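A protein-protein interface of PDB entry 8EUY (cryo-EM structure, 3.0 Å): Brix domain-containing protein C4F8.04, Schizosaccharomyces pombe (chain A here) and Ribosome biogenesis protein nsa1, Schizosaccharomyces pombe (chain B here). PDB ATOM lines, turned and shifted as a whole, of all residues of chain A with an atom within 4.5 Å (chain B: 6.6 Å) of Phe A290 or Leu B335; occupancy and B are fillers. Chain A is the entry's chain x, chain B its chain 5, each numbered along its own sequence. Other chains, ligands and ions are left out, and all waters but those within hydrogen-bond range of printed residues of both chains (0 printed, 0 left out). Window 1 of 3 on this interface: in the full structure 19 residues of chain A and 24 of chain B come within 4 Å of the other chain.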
ATOM      1  N   GLU A  77     -22.278 -18.717 -11.206  1.00  0.00           N
ATOM      2  CA  GLU A  77     -22.827 -18.115  -9.998  1.00  0.00           C
ATOM      3  C   GLU A  77     -23.042 -16.618 -10.174  1.00  0.00           C
ATOM      4  O   GLU A  77     -24.065 -16.078  -9.739  1.00  0.00           O
ATOM      5  CB  GLU A  77     -21.895 -18.381  -8.818  1.00  0.00           C
ATOM      6  CG  GLU A  77     -22.274 -19.588  -7.987  1.00  0.00           C
ATOM      7  CD  GLU A  77     -21.758 -19.496  -6.567  1.00  0.00           C
ATOM      8  OE1 GLU A  77     -20.678 -18.903  -6.364  1.00  0.00           O
ATOM      9  OE2 GLU A  77     -22.434 -20.013  -5.653  1.00  0.00           O
ATOM     10  N   VAL A 277     -20.184  -9.696   6.862  1.00  0.00           N
ATOM     11  CA  VAL A 277     -20.987  -9.663   5.646  1.00  0.00           C
ATOM     12  C   VAL A 277     -22.290 -10.389   5.939  1.00  0.00           C
ATOM     13  O   VAL A 277     -22.275 -11.506   6.469  1.00  0.00           O
ATOM     14  CB  VAL A 277     -20.260 -10.313   4.457  1.00  0.00           C
ATOM     15  CG1 VAL A 277     -21.097 -10.195   3.198  1.00  0.00           C
ATOM     16  CG2 VAL A 277     -18.902  -9.683   4.256  1.00  0.00           C
ATOM     17  N   GLN A 278     -23.409  -9.760   5.605  1.00  0.00           N
ATOM     18  CA  GLN A 278     -24.720 -10.342   5.840  1.00  0.00           C
ATOM     19  C   GLN A 278     -25.438 -10.571   4.521  1.00  0.00           C
ATOM     20  O   GLN A 278     -25.272  -9.811   3.564  1.00  0.00           O
ATOM     21  CB  GLN A 278     -25.580  -9.447   6.736  1.00  0.00           C
ATOM     22  CG  GLN A 278     -25.079  -9.321   8.156  1.00  0.00           C
ATOM     23  CD  GLN A 278     -26.151  -8.838   9.100  1.00  0.00           C
ATOM     24  OE1 GLN A 278     -27.015  -8.053   8.724  1.00  0.00           O
ATOM     25  NE2 GLN A 278     -26.100  -9.304  10.340  1.00  0.00           N
ATOM     26  N   LYS A 279     -26.229 -11.636   4.474  1.00  0.00           N
ATOM     27  CA  LYS A 279     -27.141 -11.852   3.360  1.00  0.00           C
ATOM     28  C   LYS A 279     -28.378 -10.989   3.570  1.00  0.00           C
ATOM     29  O   LYS A 279     -29.072 -11.127   4.582  1.00  0.00           O
ATOM     30  CB  LYS A 279     -27.523 -13.325   3.253  1.00  0.00           C
ATOM     31  CG  LYS A 279     -26.604 -14.145   2.376  1.00  0.00           C
ATOM     32  CD  LYS A 279     -27.270 -15.444   1.955  1.00  0.00           C
ATOM     33  CE  LYS A 279     -28.227 -15.225   0.798  1.00  0.00           C
ATOM     34  NZ  LYS A 279     -27.501 -15.002  -0.484  1.00  0.00           N
ATOM     35  N   GLU A 288     -28.558 -12.490   8.742  1.00  0.00           N
ATOM     36  CA  GLU A 288     -27.990 -13.791   8.415  1.00  0.00           C
ATOM     37  C   GLU A 288     -26.521 -13.606   8.061  1.00  0.00           C
ATOM     38  O   GLU A 288     -26.199 -12.918   7.089  1.00  0.00           O
ATOM     39  CB  GLU A 288     -28.752 -14.426   7.255  1.00  0.00           C
ATOM     40  CG  GLU A 288     -28.221 -15.761   6.803  1.00  0.00           C
ATOM     41  CD  GLU A 288     -29.165 -16.450   5.847  1.00  0.00           C
ATOM     42  OE1 GLU A 288     -30.143 -15.805   5.416  1.00  0.00           O
ATOM     43  OE2 GLU A 288     -28.936 -17.634   5.525  1.00  0.00           O
ATOM     44  N   VAL A 289     -25.639 -14.232   8.835  1.00  0.00           N
ATOM     45  CA  VAL A 289     -24.210 -13.935   8.768  1.00  0.00           C
ATOM     46  C   VAL A 289     -23.576 -14.755   7.648  1.00  0.00           C
ATOM     47  O   VAL A 289     -23.439 -15.974   7.754  1.00  0.00           O
ATOM     48  CB  VAL A 289     -23.520 -14.201  10.109  1.00  0.00           C
ATOM     49  CG1 VAL A 289     -22.021 -14.197   9.933  1.00  0.00           C
ATOM     50  CG2 VAL A 289     -23.918 -13.147  11.108  1.00  0.00           C
ATOM     51  N   PHE A 290     -23.192 -14.075   6.568  1.00  0.00           N
ATOM     52  CA  PHE A 290     -22.402 -14.713   5.523  1.00  0.00           C
ATOM     53  C   PHE A 290     -20.960 -14.897   5.974  1.00  0.00           C
ATOM     54  O   PHE A 290     -20.353 -15.946   5.734  1.00  0.00           O
ATOM     55  CB  PHE A 290     -22.474 -13.870   4.248  1.00  0.00           C
ATOM     56  CG  PHE A 290     -22.114 -14.612   2.997  1.00  0.00           C
ATOM     57  CD1 PHE A 290     -20.849 -15.140   2.818  1.00  0.00           C
ATOM     58  CD2 PHE A 290     -23.038 -14.750   1.977  1.00  0.00           C
ATOM     59  CE1 PHE A 290     -20.520 -15.812   1.664  1.00  0.00           C
ATOM     60  CE2 PHE A 290     -22.716 -15.422   0.820  1.00  0.00           C
ATOM     61  CZ  PHE A 290     -21.454 -15.953   0.663  1.00  0.00           C
ATOM     62  N   PHE A 291     -20.402 -13.890   6.638  1.00  0.00           N
ATOM     63  CA  PHE A 291     -19.036 -13.934   7.136  1.00  0.00           C
ATOM     64  C   PHE A 291     -18.964 -13.052   8.370  1.00  0.00           C
ATOM     65  O   PHE A 291     -19.491 -11.937   8.363  1.00  0.00           O
ATOM     66  CB  PHE A 291     -18.049 -13.457   6.067  1.00  0.00           C
ATOM     67  CG  PHE A 291     -16.743 -12.962   6.616  1.00  0.00           C
ATOM     68  CD1 PHE A 291     -15.753 -13.852   6.988  1.00  0.00           C
ATOM     69  CD2 PHE A 291     -16.497 -11.609   6.741  1.00  0.00           C
ATOM     70  CE1 PHE A 291     -14.554 -13.401   7.486  1.00  0.00           C
ATOM     71  CE2 PHE A 291     -15.300 -11.156   7.238  1.00  0.00           C
ATOM     72  CZ  PHE A 291     -14.326 -12.052   7.610  1.00  0.00           C
ATOM     73  N   GLY B   6     -27.050 -30.142  -2.709  1.00  0.00           N
ATOM     74  CA  GLY B   6     -27.587 -29.274  -3.737  1.00  0.00           C
ATOM     75  C   GLY B   6     -27.140 -27.843  -3.541  1.00  0.00           C
ATOM     76  O   GLY B   6     -26.754 -27.462  -2.433  1.00  0.00           O
ATOM     77  N   ASP B   7     -27.183 -27.035  -4.595  1.00  0.00           N
ATOM     78  CA  ASP B   7     -26.636 -25.688  -4.559  1.00  0.00           C
ATOM     79  C   ASP B   7     -27.686 -24.689  -5.027  1.00  0.00           C
ATOM     80  O   ASP B   7     -28.751 -25.058  -5.525  1.00  0.00           O
ATOM     81  CB  ASP B   7     -25.374 -25.578  -5.425  1.00  0.00           C
ATOM     82  CG  ASP B   7     -24.162 -26.207  -4.767  1.00  0.00           C
ATOM     83  OD1 ASP B   7     -24.306 -27.280  -4.149  1.00  0.00           O
ATOM     84  OD2 ASP B   7     -23.061 -25.632  -4.861  1.00  0.00           O
ATOM     85  N   GLU B   8     -27.367 -23.405  -4.861  1.00  0.00           N
ATOM     86  CA  GLU B   8     -28.299 -22.348  -5.237  1.00  0.00           C
ATOM     87  C   GLU B   8     -28.447 -22.204  -6.744  1.00  0.00           C
ATOM     88  O   GLU B   8     -29.431 -21.616  -7.200  1.00  0.00           O
ATOM     89  CB  GLU B   8     -27.857 -21.013  -4.640  1.00  0.00           C
ATOM     90  CG  GLU B   8     -28.557 -20.650  -3.343  1.00  0.00           C
ATOM     91  CD  GLU B   8     -28.439 -19.175  -3.013  1.00  0.00           C
ATOM     92  OE1 GLU B   8     -27.633 -18.482  -3.670  1.00  0.00           O
ATOM     93  OE2 GLU B   8     -29.152 -18.708  -2.104  1.00  0.00           O
ATOM     94  N   ILE B   9     -27.495 -22.712  -7.527  1.00  0.00           N
ATOM     95  CA  ILE B   9     -27.591 -22.668  -8.980  1.00  0.00           C
ATOM     96  C   ILE B   9     -28.098 -23.986  -9.553  1.00  0.00           C
ATOM     97  O   ILE B   9     -27.974 -24.224 -10.758  1.00  0.00           O
ATOM     98  CB  ILE B   9     -26.252 -22.270  -9.620  1.00  0.00           C
ATOM     99  CG1 ILE B   9     -25.171 -23.299  -9.299  1.00  0.00           C
ATOM    100  CG2 ILE B   9     -25.828 -20.894  -9.145  1.00  0.00           C
ATOM    101  CD1 ILE B   9     -23.824 -22.940  -9.863  1.00  0.00           C
ATOM    102  N   LYS B 273     -29.338 -18.144  12.813  1.00  0.00           N
ATOM    103  CA  LYS B 273     -28.784 -17.408  11.684  1.00  0.00           C
ATOM    104  C   LYS B 273     -27.405 -16.828  11.963  1.00  0.00           C
ATOM    105  O   LYS B 273     -26.766 -16.328  11.035  1.00  0.00           O
ATOM    106  CB  LYS B 273     -29.730 -16.278  11.276  1.00  0.00           C
ATOM    107  CG  LYS B 273     -31.043 -16.737  10.680  1.00  0.00           C
ATOM    108  CD  LYS B 273     -31.728 -15.588   9.969  1.00  0.00           C
ATOM    109  CE  LYS B 273     -32.970 -16.041   9.235  1.00  0.00           C
ATOM    110  NZ  LYS B 273     -33.796 -14.878   8.814  1.00  0.00           N
ATOM    111  N   LYS B 295     -18.592 -21.763  10.235  1.00  0.00           N
ATOM    112  CA  LYS B 295     -18.687 -20.351   9.910  1.00  0.00           C
ATOM    113  C   LYS B 295     -19.827 -20.140   8.925  1.00  0.00           C
ATOM    114  O   LYS B 295     -20.171 -21.036   8.153  1.00  0.00           O
ATOM    115  CB  LYS B 295     -17.373 -19.834   9.319  1.00  0.00           C
ATOM    116  CG  LYS B 295     -16.136 -20.313  10.060  1.00  0.00           C
ATOM    117  CD  LYS B 295     -16.029 -19.664  11.427  1.00  0.00           C
ATOM    118  CE  LYS B 295     -14.714 -20.004  12.100  1.00  0.00           C
ATOM    119  NZ  LYS B 295     -14.710 -21.390  12.636  1.00  0.00           N
ATOM    120  N   GLY B 296     -20.438 -18.962   8.977  1.00  0.00           N
ATOM    121  CA  GLY B 296     -21.545 -18.676   8.087  1.00  0.00           C
ATOM    122  C   GLY B 296     -22.813 -19.397   8.489  1.00  0.00           C
ATOM    123  O   GLY B 296     -22.760 -20.522   8.991  1.00  0.00           O
ATOM    124  N   ALA B 297     -23.958 -18.770   8.259  1.00  0.00           N
ATOM    125  CA  ALA B 297     -25.216 -19.331   8.723  1.00  0.00           C
ATOM    126  C   ALA B 297     -25.498 -20.648   8.012  1.00  0.00           C
ATOM    127  O   ALA B 297     -25.441 -20.702   6.776  1.00  0.00           O
ATOM    128  CB  ALA B 297     -26.358 -18.350   8.479  1.00  0.00           C
ATOM    129  N   GLY B 312     -23.467 -24.518   4.921  1.00  0.00           N
ATOM    130  CA  GLY B 312     -23.904 -23.161   5.150  1.00  0.00           C
ATOM    131  C   GLY B 312     -23.295 -22.175   4.187  1.00  0.00           C
ATOM    132  O   GLY B 312     -22.889 -22.526   3.080  1.00  0.00           O
ATOM    133  N   LEU B 313     -23.229 -20.922   4.631  1.00  0.00           N
ATOM    134  CA  LEU B 313     -22.757 -19.823   3.799  1.00  0.00           C
ATOM    135  C   LEU B 313     -21.240 -19.731   3.726  1.00  0.00           C
ATOM    136  O   LEU B 313     -20.725 -18.883   2.990  1.00  0.00           O
ATOM    137  CB  LEU B 313     -23.331 -18.501   4.307  1.00  0.00           C
ATOM    138  CG  LEU B 313     -24.838 -18.328   4.135  1.00  0.00           C
ATOM    139  CD1 LEU B 313     -25.281 -16.972   4.642  1.00  0.00           C
ATOM    140  CD2 LEU B 313     -25.216 -18.503   2.681  1.00  0.00           C
ATOM    141  N   ASP B 314     -20.513 -20.566   4.465  1.00  0.00           N
ATOM    142  CA  ASP B 314     -19.067 -20.637   4.307  1.00  0.00           C
ATOM    143  C   ASP B 314     -18.652 -21.492   3.120  1.00  0.00           C
ATOM    144  O   ASP B 314     -17.450 -21.706   2.925  1.00  0.00           O
ATOM    145  CB  ASP B 314     -18.414 -21.177   5.580  1.00  0.00           C
ATOM    146  CG  ASP B 314     -18.941 -22.539   5.975  1.00  0.00           C
ATOM    147  OD1 ASP B 314     -20.020 -22.929   5.485  1.00  0.00           O
ATOM    148  OD2 ASP B 314     -18.280 -23.218   6.787  1.00  0.00           O
ATOM    149  N   ARG B 315     -19.613 -21.976   2.331  1.00  0.00           N
ATOM    150  CA  ARG B 315     -19.349 -22.791   1.146  1.00  0.00           C
ATOM    151  C   ARG B 315     -18.542 -24.034   1.501  1.00  0.00           C
ATOM    152  O   ARG B 315     -17.684 -24.478   0.738  1.00  0.00           O
ATOM    153  CB  ARG B 315     -18.647 -21.974   0.061  1.00  0.00           C
ATOM    154  CG  ARG B 315     -19.142 -20.546  -0.034  1.00  0.00           C
ATOM    155  CD  ARG B 315     -19.001 -19.989  -1.428  1.00  0.00           C
ATOM    156  NE  ARG B 315     -19.402 -18.590  -1.481  1.00  0.00           N
ATOM    157  CZ  ARG B 315     -20.105 -18.051  -2.465  1.00  0.00           C
ATOM    158  NH1 ARG B 315     -20.499 -18.768  -3.504  1.00  0.00           N
ATOM    159  NH2 ARG B 315     -20.420 -16.761  -2.406  1.00  0.00           N
ATOM    160  N   ILE B 332     -16.790 -26.621  -1.273  1.00  0.00           N
ATOM    161  CA  ILE B 332     -17.679 -26.962  -2.375  1.00  0.00           C
ATOM    162  C   ILE B 332     -17.875 -25.805  -3.346  1.00  0.00           C
ATOM    163  O   ILE B 332     -18.788 -25.845  -4.169  1.00  0.00           O
ATOM    164  CB  ILE B 332     -19.037 -27.463  -1.850  1.00  0.00           C
ATOM    165  CG1 ILE B 332     -19.635 -26.430  -0.900  1.00  0.00           C
ATOM    166  CG2 ILE B 332     -18.875 -28.802  -1.153  1.00  0.00           C
ATOM    167  CD1 ILE B 332     -21.050 -26.716  -0.510  1.00  0.00           C
ATOM    168  N   LYS B 333     -17.051 -24.764  -3.252  1.00  0.00           N
ATOM    169  CA  LYS B 333     -17.019 -23.681  -4.232  1.00  0.00           C
ATOM    170  C   LYS B 333     -18.324 -22.896  -4.313  1.00  0.00           C
ATOM    171  O   LYS B 333     -18.352 -21.706  -3.986  1.00  0.00           O
ATOM    172  CB  LYS B 333     -16.651 -24.230  -5.612  1.00  0.00           C
ATOM    173  CG  LYS B 333     -15.252 -24.809  -5.671  1.00  0.00           C
ATOM    174  CD  LYS B 333     -14.992 -25.522  -6.978  1.00  0.00           C
ATOM    175  CE  LYS B 333     -13.738 -26.371  -6.883  1.00  0.00           C
ATOM    176  NZ  LYS B 333     -13.819 -27.343  -5.760  1.00  0.00           N
ATOM    177  N   ALA B 334     -19.401 -23.530  -4.761  1.00  0.00           N
ATOM    178  CA  ALA B 334     -20.649 -22.816  -4.981  1.00  0.00           C
ATOM    179  C   ALA B 334     -21.528 -22.848  -3.734  1.00  0.00           C
ATOM    180  O   ALA B 334     -21.426 -23.740  -2.890  1.00  0.00           O
ATOM    181  CB  ALA B 334     -21.402 -23.397  -6.175  1.00  0.00           C
ATOM    182  N   LEU B 335     -22.404 -21.855  -3.636  1.00  0.00           N
ATOM    183  CA  LEU B 335     -23.214 -21.659  -2.439  1.00  0.00           C
ATOM    184  C   LEU B 335     -24.236 -22.779  -2.297  1.00  0.00           C
ATOM    185  O   LEU B 335     -25.064 -22.968  -3.197  1.00  0.00           O
ATOM    186  CB  LEU B 335     -23.915 -20.308  -2.506  1.00  0.00           C
ATOM    187  CG  LEU B 335     -24.187 -19.597  -1.181  1.00  0.00           C
ATOM    188  CD1 LEU B 335     -22.886 -19.162  -0.537  1.00  0.00           C
ATOM    189  CD2 LEU B 335     -25.101 -18.407  -1.397  1.00  0.00           C
ATOM    190  N   PRO B 336     -24.234 -23.524  -1.197  1.00  0.00           N
ATOM    191  CA  PRO B 336     -25.146 -24.657  -1.048  1.00  0.00           C
ATOM    192  C   PRO B 336     -26.505 -24.228  -0.506  1.00  0.00           C
ATOM    193  O   PRO B 336     -26.685 -23.118  -0.003  1.00  0.00           O
ATOM    194  CB  PRO B 336     -24.416 -25.544  -0.038  1.00  0.00           C
ATOM    195  CG  PRO B 336     -23.705 -24.575   0.823  1.00  0.00           C
ATOM    196  CD  PRO B 336     -23.338 -23.390  -0.037  1.00  0.00           C
ATOM    197  N   THR B 337     -27.465 -25.143  -0.623  1.00  0.00           N
ATOM    198  CA  THR B 337     -28.812 -24.894  -0.127  1.00  0.00           C
ATOM    199  C   THR B 337     -29.319 -26.068   0.699  1.00  0.00           C
ATOM    200  O   THR B 337     -30.184 -25.895   1.563  1.00  0.00           O
ATOM    201  CB  THR B 337     -29.766 -24.610  -1.287  1.00  0.00           C
ATOM    202  OG1 THR B 337     -29.132 -23.730  -2.223  1.00  0.00           O
ATOM    203  CG2 THR B 337     -31.033 -23.954  -0.780  1.00  0.00           C
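OE1 of Glu A77 lies within salt-bridge range of NH1 of Arg B315, at 2.9 Å. N of Leu B335 sits at hydrogen-bond distance from OE2 of Glu A77, at 2.7 Å. O of Lys B273 lies within hydrogen-bond range of N of Val A289, 3.2 Å away. The backbone carbonyl oxygen of Val A289 lies within hydrogen-bond range of the backbone NH of Ala B297, 2.9 Å away.
N of Phe A290 sits at hydrogen-bond distance from O of Val A277 (2.7 Å). The backbone NH (N) of Lys A279 sits at hydrogen-bond distance from the backbone carbonyl oxygen (O) of Glu A288, 2.9 Å away. O of Leu B335 sits at hydrogen-bond distance from N of Glu B8 (2.9 Å). The backbone carbonyl oxygen (O) of Ala B297 lies within hydrogen-bond range of the backbone NH (N) of Leu B313. O of Arg B315 lies within hydrogen-bond range of N of Ile B332, 3.1 Å away.
Among the printed residues, merely in contact across the chains: Glu A77 with Ile B9, Glu A77 with Ala B334, Lys A279 with Leu B313, Glu A288 with Lys B273, Glu A288 with Ala B297, Glu A288 with Leu B313, Val A289 with Gly B296, Val A289 with Leu B313, Phe A290 with Gly B296, Phe A290 with Leu B313, Phe A290 with Arg B315 and Phe A290 with Leu B335.
Of chain A, only Glu A77 and Phe A290 come within 4 Å of Leu B335. Of the printed residues of chain A, Ala B334 touches Glu A77 (3.4 Å). Printed residues of chain A within 4 Å of Ile B9: Glu A77. Printed residues of chain A within 4 Å of Lys B273: Glu A288 and Val A289. Of the printed residues of chain A, Ala B297 touches Glu A288 (3.6 Å) and Val A289 (2.9 Å). The nearest residue of chain B that does not touch Phe A290 is Asp B314 (4.8 Å). The nearest residue of chain A that does not touch Leu B335 is Lys A279 (4.3 Å). The nearest printed residue of chain A that does not touch Ala B297 is Phe A290 (5.0 Å).
Of the 8 printed residues of chain A, 5 touch a printed residue of chain B. Of the 18 printed residues of chain B, 8 touch a printed residue of chain A. Hydrophobic or aromatic side chains of chain B within 4 Å of the printed part of chain A: Ile B9, Ala B297, Leu B313, Ala B334 and Leu B335.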
